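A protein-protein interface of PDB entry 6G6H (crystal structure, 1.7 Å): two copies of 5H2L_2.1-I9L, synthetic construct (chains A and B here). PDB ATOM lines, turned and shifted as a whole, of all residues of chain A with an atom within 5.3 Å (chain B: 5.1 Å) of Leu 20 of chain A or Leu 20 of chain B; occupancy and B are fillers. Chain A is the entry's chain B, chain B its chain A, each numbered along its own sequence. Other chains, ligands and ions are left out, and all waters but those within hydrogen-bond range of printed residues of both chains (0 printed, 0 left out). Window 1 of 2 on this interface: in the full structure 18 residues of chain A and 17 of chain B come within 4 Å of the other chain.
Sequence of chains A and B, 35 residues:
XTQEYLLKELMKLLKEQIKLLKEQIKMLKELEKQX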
ATOM      1  N   LEU A  13     -27.277 -16.791 -24.511  1.00  0.00           N
ATOM      2  CA  LEU A  13     -27.022 -15.441 -25.004  1.00  0.00           C
ATOM      3  C   LEU A  13     -26.937 -14.432 -23.856  1.00  0.00           C
ATOM      4  O   LEU A  13     -26.140 -13.481 -23.916  1.00  0.00           O
ATOM      5  CB  LEU A  13     -28.103 -15.049 -26.015  1.00  0.00           C
ATOM      6  CG  LEU A  13     -28.172 -15.901 -27.299  1.00  0.00           C
ATOM      7  CD1 LEU A  13     -29.468 -15.667 -28.054  1.00  0.00           C
ATOM      8  CD2 LEU A  13     -26.997 -15.587 -28.196  1.00  0.00           C
ATOM      9  N   GLU A  16     -23.532 -14.641 -22.322  1.00  0.00           N
ATOM     10  CA  GLU A  16     -22.555 -13.901 -23.119  1.00  0.00           C
ATOM     11  C   GLU A  16     -22.624 -12.401 -22.840  1.00  0.00           C
ATOM     12  O   GLU A  16     -21.596 -11.716 -22.850  1.00  0.00           O
ATOM     13  CB  GLU A  16     -22.763 -14.174 -24.608  1.00  0.00           C
ATOM     14  CG  GLU A  16     -22.501 -15.614 -25.018  1.00  0.00           C
ATOM     15  CD  GLU A  16     -22.693 -15.846 -26.508  1.00  0.00           C
ATOM     16  OE1 GLU A  16     -22.319 -14.955 -27.304  1.00  0.00           O
ATOM     17  OE2 GLU A  16     -23.222 -16.917 -26.882  1.00  0.00           O
ATOM     18  N   GLN A  17     -23.824 -11.862 -22.597  1.00  0.00           N
ATOM     19  CA  GLN A  17     -23.915 -10.440 -22.279  1.00  0.00           C
ATOM     20  C   GLN A  17     -23.223 -10.122 -20.955  1.00  0.00           C
ATOM     21  O   GLN A  17     -22.618  -9.052 -20.802  1.00  0.00           O
ATOM     22  CB  GLN A  17     -25.386 -10.001 -22.218  1.00  0.00           C
ATOM     23  CG  GLN A  17     -26.075  -9.878 -23.577  1.00  0.00           C
ATOM     24  CD  GLN A  17     -27.395  -9.121 -23.472  1.00  0.00           C
ATOM     25  OE1 GLN A  17     -28.424  -9.710 -23.164  1.00  0.00           O
ATOM     26  NE2 GLN A  17     -27.360  -7.808 -23.706  1.00  0.00           N
ATOM     27  N   ILE A  18     -23.331 -11.026 -19.973  1.00  0.00           N
ATOM     28  CA  ILE A  18     -22.655 -10.826 -18.690  1.00  0.00           C
ATOM     29  C   ILE A  18     -21.146 -10.773 -18.894  1.00  0.00           C
ATOM     30  O   ILE A  18     -20.456  -9.921 -18.322  1.00  0.00           O
ATOM     31  CB  ILE A  18     -23.040 -11.938 -17.699  1.00  0.00           C
ATOM     32  CG1 ILE A  18     -24.502 -11.790 -17.270  1.00  0.00           C
ATOM     33  CG2 ILE A  18     -22.121 -11.913 -16.477  1.00  0.00           C
ATOM     34  CD1 ILE A  18     -24.985 -12.949 -16.429  1.00  0.00           C
ATOM     35  N   LYS A  19     -20.616 -11.696 -19.700  1.00  0.00           N
ATOM     36  CA  LYS A  19     -19.180 -11.710 -19.987  1.00  0.00           C
ATOM     37  C   LYS A  19     -18.718 -10.366 -20.553  1.00  0.00           C
ATOM     38  O   LYS A  19     -17.692  -9.820 -20.129  1.00  0.00           O
ATOM     39  CB  LYS A  19     -18.857 -12.852 -20.956  1.00  0.00           C
ATOM     40  CG  LYS A  19     -17.419 -12.935 -21.451  1.00  0.00           C
ATOM     41  N   LEU A  20     -19.494  -9.795 -21.479  1.00  0.00           N
ATOM     42  CA  LEU A  20     -19.114  -8.522 -22.097  1.00  0.00           C
ATOM     43  C   LEU A  20     -19.212  -7.356 -21.105  1.00  0.00           C
ATOM     44  O   LEU A  20     -18.374  -6.447 -21.134  1.00  0.00           O
ATOM     45  CB  LEU A  20     -19.990  -8.249 -23.326  1.00  0.00           C
ATOM     46  CG  LEU A  20     -19.939  -9.171 -24.556  1.00  0.00           C
ATOM     47  CD1 LEU A  20     -20.974  -8.732 -25.588  1.00  0.00           C
ATOM     48  CD2 LEU A  20     -18.550  -9.158 -25.187  1.00  0.00           C
ATOM     49  N   LEU A  21     -20.227  -7.355 -20.229  1.00  0.00           N
ATOM     50  CA  LEU A  21     -20.342  -6.291 -19.229  1.00  0.00           C
ATOM     51  C   LEU A  21     -19.133  -6.278 -18.300  1.00  0.00           C
ATOM     52  O   LEU A  21     -18.651  -5.205 -17.901  1.00  0.00           O
ATOM     53  CB  LEU A  21     -21.641  -6.456 -18.413  1.00  0.00           C
ATOM     54  CG  LEU A  21     -22.932  -6.024 -19.112  1.00  0.00           C
ATOM     55  CD1 LEU A  21     -24.148  -6.458 -18.311  1.00  0.00           C
ATOM     56  CD2 LEU A  21     -22.938  -4.519 -19.298  1.00  0.00           C
ATOM     57  N   LYS A  22     -18.625  -7.459 -17.939  1.00  0.00           N
ATOM     58  CA  LYS A  22     -17.432  -7.508 -17.098  1.00  0.00           C
ATOM     59  C   LYS A  22     -16.228  -6.889 -17.804  1.00  0.00           C
ATOM     60  O   LYS A  22     -15.428  -6.196 -17.170  1.00  0.00           O
ATOM     61  CB  LYS A  22     -17.138  -8.950 -16.668  1.00  0.00           C
ATOM     62  CG  LYS A  22     -18.145  -9.531 -15.675  1.00  0.00           C
ATOM     63  CD  LYS A  22     -17.858 -11.017 -15.433  1.00  0.00           C
ATOM     64  CE  LYS A  22     -18.714 -11.573 -14.303  1.00  0.00           C
ATOM     65  NZ  LYS A  22     -18.373 -13.001 -14.033  1.00  0.00           N
ATOM     66  N   GLU A  23     -16.091  -7.100 -19.118  1.00  0.00           N
ATOM     67  CA  GLU A  23     -15.012  -6.456 -19.864  1.00  0.00           C
ATOM     68  C   GLU A  23     -15.201  -4.943 -19.933  1.00  0.00           C
ATOM     69  O   GLU A  23     -14.220  -4.188 -19.919  1.00  0.00           O
ATOM     70  CB  GLU A  23     -14.913  -7.045 -21.273  1.00  0.00           C
ATOM     71  CG  GLU A  23     -14.418  -8.479 -21.317  1.00  0.00           C
ATOM     72  N   GLN A  24     -16.456  -4.480 -20.025  1.00  0.00           N
ATOM     73  CA  GLN A  24     -16.724  -3.043 -20.042  1.00  0.00           C
ATOM     74  C   GLN A  24     -16.296  -2.386 -18.730  1.00  0.00           C
ATOM     75  O   GLN A  24     -15.718  -1.295 -18.737  1.00  0.00           O
ATOM     76  CB  GLN A  24     -18.216  -2.793 -20.334  1.00  0.00           C
ATOM     77  CG  GLN A  24     -18.619  -3.222 -21.755  1.00  0.00           C
ATOM     78  CD  GLN A  24     -20.135  -3.298 -21.946  1.00  0.00           C
ATOM     79  OE1 GLN A  24     -20.654  -4.253 -22.528  1.00  0.00           O
ATOM     80  NE2 GLN A  24     -20.843  -2.287 -21.457  1.00  0.00           N
ATOM     81  N   ILE A  25     -16.548  -3.048 -17.597  1.00  0.00           N
ATOM     82  CA  ILE A  25     -16.121  -2.515 -16.300  1.00  0.00           C
ATOM     83  C   ILE A  25     -14.607  -2.342 -16.263  1.00  0.00           C
ATOM     84  O   ILE A  25     -14.090  -1.340 -15.752  1.00  0.00           O
ATOM     85  CB  ILE A  25     -16.624  -3.431 -15.162  1.00  0.00           C
ATOM     86  CG1 ILE A  25     -18.139  -3.279 -15.007  1.00  0.00           C
ATOM     87  CG2 ILE A  25     -15.903  -3.124 -13.841  1.00  0.00           C
ATOM     88  CD1 ILE A  25     -18.802  -4.340 -14.130  1.00  0.00           C
ATOM     89  N   LEU B  13     -17.437  -3.382 -27.722  1.00  0.00           N
ATOM     90  CA  LEU B  13     -18.218  -4.204 -26.793  1.00  0.00           C
ATOM     91  C   LEU B  13     -19.702  -3.848 -26.840  1.00  0.00           C
ATOM     92  O   LEU B  13     -20.563  -4.739 -26.768  1.00  0.00           O
ATOM     93  CB  LEU B  13     -17.678  -4.062 -25.363  1.00  0.00           C
ATOM     94  CG  LEU B  13     -16.247  -4.589 -25.127  1.00  0.00           C
ATOM     95  CD1 LEU B  13     -15.588  -3.990 -23.873  1.00  0.00           C
ATOM     96  CD2 LEU B  13     -16.211  -6.113 -25.073  1.00  0.00           C
ATOM     97  N   GLU B  16     -21.195  -5.430 -29.881  1.00  0.00           N
ATOM     98  CA  GLU B  16     -21.434  -6.854 -29.655  1.00  0.00           C
ATOM     99  C   GLU B  16     -22.683  -7.086 -28.808  1.00  0.00           C
ATOM    100  O   GLU B  16     -23.389  -8.075 -29.014  1.00  0.00           O
ATOM    101  CB  GLU B  16     -20.223  -7.501 -28.986  1.00  0.00           C
ATOM    102  CG  GLU B  16     -19.019  -7.690 -29.909  1.00  0.00           C
ATOM    103  CD  GLU B  16     -17.872  -8.350 -29.178  1.00  0.00           C
ATOM    104  OE1 GLU B  16     -17.165  -7.647 -28.435  1.00  0.00           O
ATOM    105  OE2 GLU B  16     -17.693  -9.574 -29.322  1.00  0.00           O
ATOM    106  N   GLN B  17     -22.954  -6.201 -27.833  1.00  0.00           N
ATOM    107  CA  GLN B  17     -24.181  -6.319 -27.038  1.00  0.00           C
ATOM    108  C   GLN B  17     -25.418  -6.191 -27.915  1.00  0.00           C
ATOM    109  O   GLN B  17     -26.397  -6.931 -27.741  1.00  0.00           O
ATOM    110  CB  GLN B  17     -24.213  -5.247 -25.941  1.00  0.00           C
ATOM    111  CG  GLN B  17     -23.152  -5.397 -24.864  1.00  0.00           C
ATOM    112  CD  GLN B  17     -23.554  -6.358 -23.770  1.00  0.00           C
ATOM    113  OE1 GLN B  17     -24.443  -7.192 -23.953  1.00  0.00           O
ATOM    114  NE2 GLN B  17     -22.878  -6.266 -22.624  1.00  0.00           N
ATOM    115  N   ILE B  18     -25.401  -5.233 -28.844  1.00  0.00           N
ATOM    116  CA  ILE B  18     -26.531  -5.026 -29.748  1.00  0.00           C
ATOM    117  C   ILE B  18     -26.786  -6.271 -30.592  1.00  0.00           C
ATOM    118  O   ILE B  18     -27.941  -6.673 -30.795  1.00  0.00           O
ATOM    119  CB  ILE B  18     -26.278  -3.785 -30.625  1.00  0.00           C
ATOM    120  CG1 ILE B  18     -26.401  -2.509 -29.789  1.00  0.00           C
ATOM    121  CG2 ILE B  18     -27.225  -3.746 -31.819  1.00  0.00           C
ATOM    122  CD1 ILE B  18     -25.792  -1.281 -30.467  1.00  0.00           C
ATOM    123  N   LYS B  19     -25.719  -6.886 -31.113  1.00  0.00           N
ATOM    124  CA  LYS B  19     -25.854  -8.120 -31.891  1.00  0.00           C
ATOM    125  C   LYS B  19     -26.548  -9.215 -31.082  1.00  0.00           C
ATOM    126  O   LYS B  19     -27.439  -9.907 -31.594  1.00  0.00           O
ATOM    127  CB  LYS B  19     -24.466  -8.581 -32.372  1.00  0.00           C
ATOM    128  CG  LYS B  19     -24.444  -9.899 -33.170  1.00  0.00           C
ATOM    129  CD  LYS B  19     -25.104  -9.756 -34.526  1.00  0.00           C
ATOM    130  CE  LYS B  19     -24.683 -10.883 -35.463  1.00  0.00           C
ATOM    131  NZ  LYS B  19     -24.951 -12.221 -34.890  1.00  0.00           N
ATOM    132  N   LEU B  20     -26.153  -9.385 -29.815  1.00  0.00           N
ATOM    133  CA  LEU B  20     -26.770 -10.416 -28.979  1.00  0.00           C
ATOM    134  C   LEU B  20     -28.247 -10.127 -28.739  1.00  0.00           C
ATOM    135  O   LEU B  20     -29.076 -11.052 -28.752  1.00  0.00           O
ATOM    136  CB  LEU B  20     -26.016 -10.537 -27.648  1.00  0.00           C
ATOM    137  CG  LEU B  20     -24.594 -11.105 -27.787  1.00  0.00           C
ATOM    138  CD1 LEU B  20     -23.828 -10.963 -26.486  1.00  0.00           C
ATOM    139  CD2 LEU B  20     -24.662 -12.564 -28.186  1.00  0.00           C
ATOM    140  N   LEU B  21     -28.602  -8.854 -28.518  1.00  0.00           N
ATOM    141  CA  LEU B  21     -30.017  -8.522 -28.337  1.00  0.00           C
ATOM    142  C   LEU B  21     -30.829  -8.869 -29.585  1.00  0.00           C
ATOM    143  O   LEU B  21     -31.978  -9.313 -29.479  1.00  0.00           O
ATOM    144  CB  LEU B  21     -30.186  -7.043 -27.987  1.00  0.00           C
ATOM    145  CG  LEU B  21     -29.718  -6.572 -26.603  1.00  0.00           C
ATOM    146  CD1 LEU B  21     -29.784  -5.047 -26.505  1.00  0.00           C
ATOM    147  CD2 LEU B  21     -30.570  -7.209 -25.510  1.00  0.00           C
ATOM    148  N   LYS B  22     -30.247  -8.690 -30.779  1.00  0.00           N
ATOM    149  CA  LYS B  22     -30.975  -9.024 -32.002  1.00  0.00           C
ATOM    150  C   LYS B  22     -31.139 -10.532 -32.159  1.00  0.00           C
ATOM    151  O   LYS B  22     -32.168 -11.003 -32.662  1.00  0.00           O
ATOM    152  CB  LYS B  22     -30.269  -8.426 -33.227  1.00  0.00           C
ATOM    153  CG  LYS B  22     -30.342  -6.897 -33.276  1.00  0.00           C
ATOM    154  CD  LYS B  22     -29.637  -6.353 -34.520  1.00  0.00           C
ATOM    155  CE  LYS B  22     -29.640  -4.836 -34.537  1.00  0.00           C
ATOM    156  NZ  LYS B  22     -28.764  -4.325 -35.642  1.00  0.00           N
ATOM    157  N   GLU B  23     -30.140 -11.303 -31.730  1.00  0.00           N
ATOM    158  CA  GLU B  23     -30.264 -12.754 -31.758  1.00  0.00           C
ATOM    159  C   GLU B  23     -31.340 -13.227 -30.790  1.00  0.00           C
ATOM    160  O   GLU B  23     -32.068 -14.181 -31.089  1.00  0.00           O
ATOM    161  CB  GLU B  23     -28.922 -13.410 -31.429  1.00  0.00           C
ATOM    162  CG  GLU B  23     -27.789 -13.095 -32.413  1.00  0.00           C
ATOM    163  CD  GLU B  23     -27.957 -13.762 -33.768  1.00  0.00           C
ATOM    164  OE1 GLU B  23     -28.602 -14.829 -33.853  1.00  0.00           O
ATOM    165  OE2 GLU B  23     -27.432 -13.211 -34.755  1.00  0.00           O
ATOM    166  N   GLN B  24     -31.465 -12.566 -29.630  1.00  0.00           N
ATOM    167  CA  GLN B  24     -32.520 -12.931 -28.680  1.00  0.00           C
ATOM    168  C   GLN B  24     -33.909 -12.684 -29.268  1.00  0.00           C
ATOM    169  O   GLN B  24     -34.842 -13.467 -29.034  1.00  0.00           O
ATOM    170  CB  GLN B  24     -32.332 -12.155 -27.366  1.00  0.00           C
ATOM    171  CG  GLN B  24     -31.088 -12.572 -26.565  1.00  0.00           C
ATOM    172  CD  GLN B  24     -30.721 -11.586 -25.460  1.00  0.00           C
ATOM    173  OE1 GLN B  24     -31.451 -10.637 -25.196  1.00  0.00           O
ATOM    174  NE2 GLN B  24     -29.574 -11.804 -24.822  1.00  0.00           N
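OE1 of Gln 17 of chain B sits at hydrogen-bond distance from NE2 of Gln 17 of chain A (3.0 Å). OE1 of Gln 24 of chain A lies within hydrogen-bond range of NE2 of Gln 17 of chain B. NE2 of Gln 24 of chain B is in hydrogen-bond range of OE1 of Gln 17 of chain A, 2.9 Å away.
The side-chain amide oxygen (OE1) of Gln 24 of chain A sits close to the backbone carbonyl oxygen (O) of Leu 20 of chain A.
Leu 20 of chain B touches Leu 13 of chain A (CD2 to CD2, 3.8 Å). NE2 of Gln 24 of chain B touches CB of Leu 13 of chain A, 3.8 Å away. CG of Gln 17 of chain A touches CD1 of Leu 20 of chain B (3.8 Å). NE2 of Gln 17 of chain A touches CD2 of Leu 21 of chain B, 3.7 Å away. Leu 20 of chain A touches Leu 13 of chain B (CD2 to CD2, 3.8 Å). CB of Glu 16 of chain B touches CD1 of Leu 20 of chain A (3.7 Å). Gln 17 of chain B touches Leu 20 of chain A. CD1 of Leu 20 of chain A touches CD1 of Leu 20 of chain B, 3.7 Å away. Leu 21 of chain A touches Gln 17 of chain B. Gln 24 of chain A touches Leu 13 of chain B.
Leu 20 of chain A touches just these residues of chain B: Leu 13, Glu 16, Gln 17 and Leu 20. Printed residues of chain A within 4 Å of Leu 13 of chain B: Leu 20 and Gln 24. Leu 20 of chain B touches just these residues of chain A: Leu 13, Glu 16, Gln 17 and Leu 20. Printed residues of chain A within 4 Å of Leu 21 of chain B: Gln 17. Glu 23 of chain B touches none of the printed residues of chain A. Printed residues of chain A within 4 Å of Gln 24 of chain B: Leu 13 and Gln 17. The nearest printed residue of chain B that does not touch Leu 20 of chain A is Ile 18 of chain B (6.5 Å). The nearest printed residue of chain A that does not touch Gln 17 of chain B is Glu 16 of chain A (5.5 Å).
Of the 11 printed residues of chain A, 6 touch a printed residue of chain B. Hydrophobic or aromatic side chains of chain A within 4 Å of the printed part of chain B: Leu 13, Leu 20 and Leu 21. Hydrophobic or aromatic side chains of chain B that line the printed part of chain A: Leu 13, Leu 20 and Leu 21. Among the printed residues, no Asp or Glu carboxylate lies within 4 Å of a Lys or Arg side-chain nitrogen of the other chain.
Leu 13 of chain A touches Leu 20 of chain B, and with the chains exchanged Leu 20 of chain A touches Leu 13 of chain B. Leu 13 of chain A touches Gln 24 of chain B, and with the chains exchanged Gln 24 of chain A touches Leu 13 of chain B. Gln 17 of chain A touches Gln 24 of chain B, and with the chains exchanged Gln 24 of chain A touches Gln 17 of chain B. Leu 20 of chain A touches its own counterpart, Leu 20 of chain B. Positions printed for both chains: 13, 16, 17, 18, 19, 20, 21, 22, 23 and 24.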
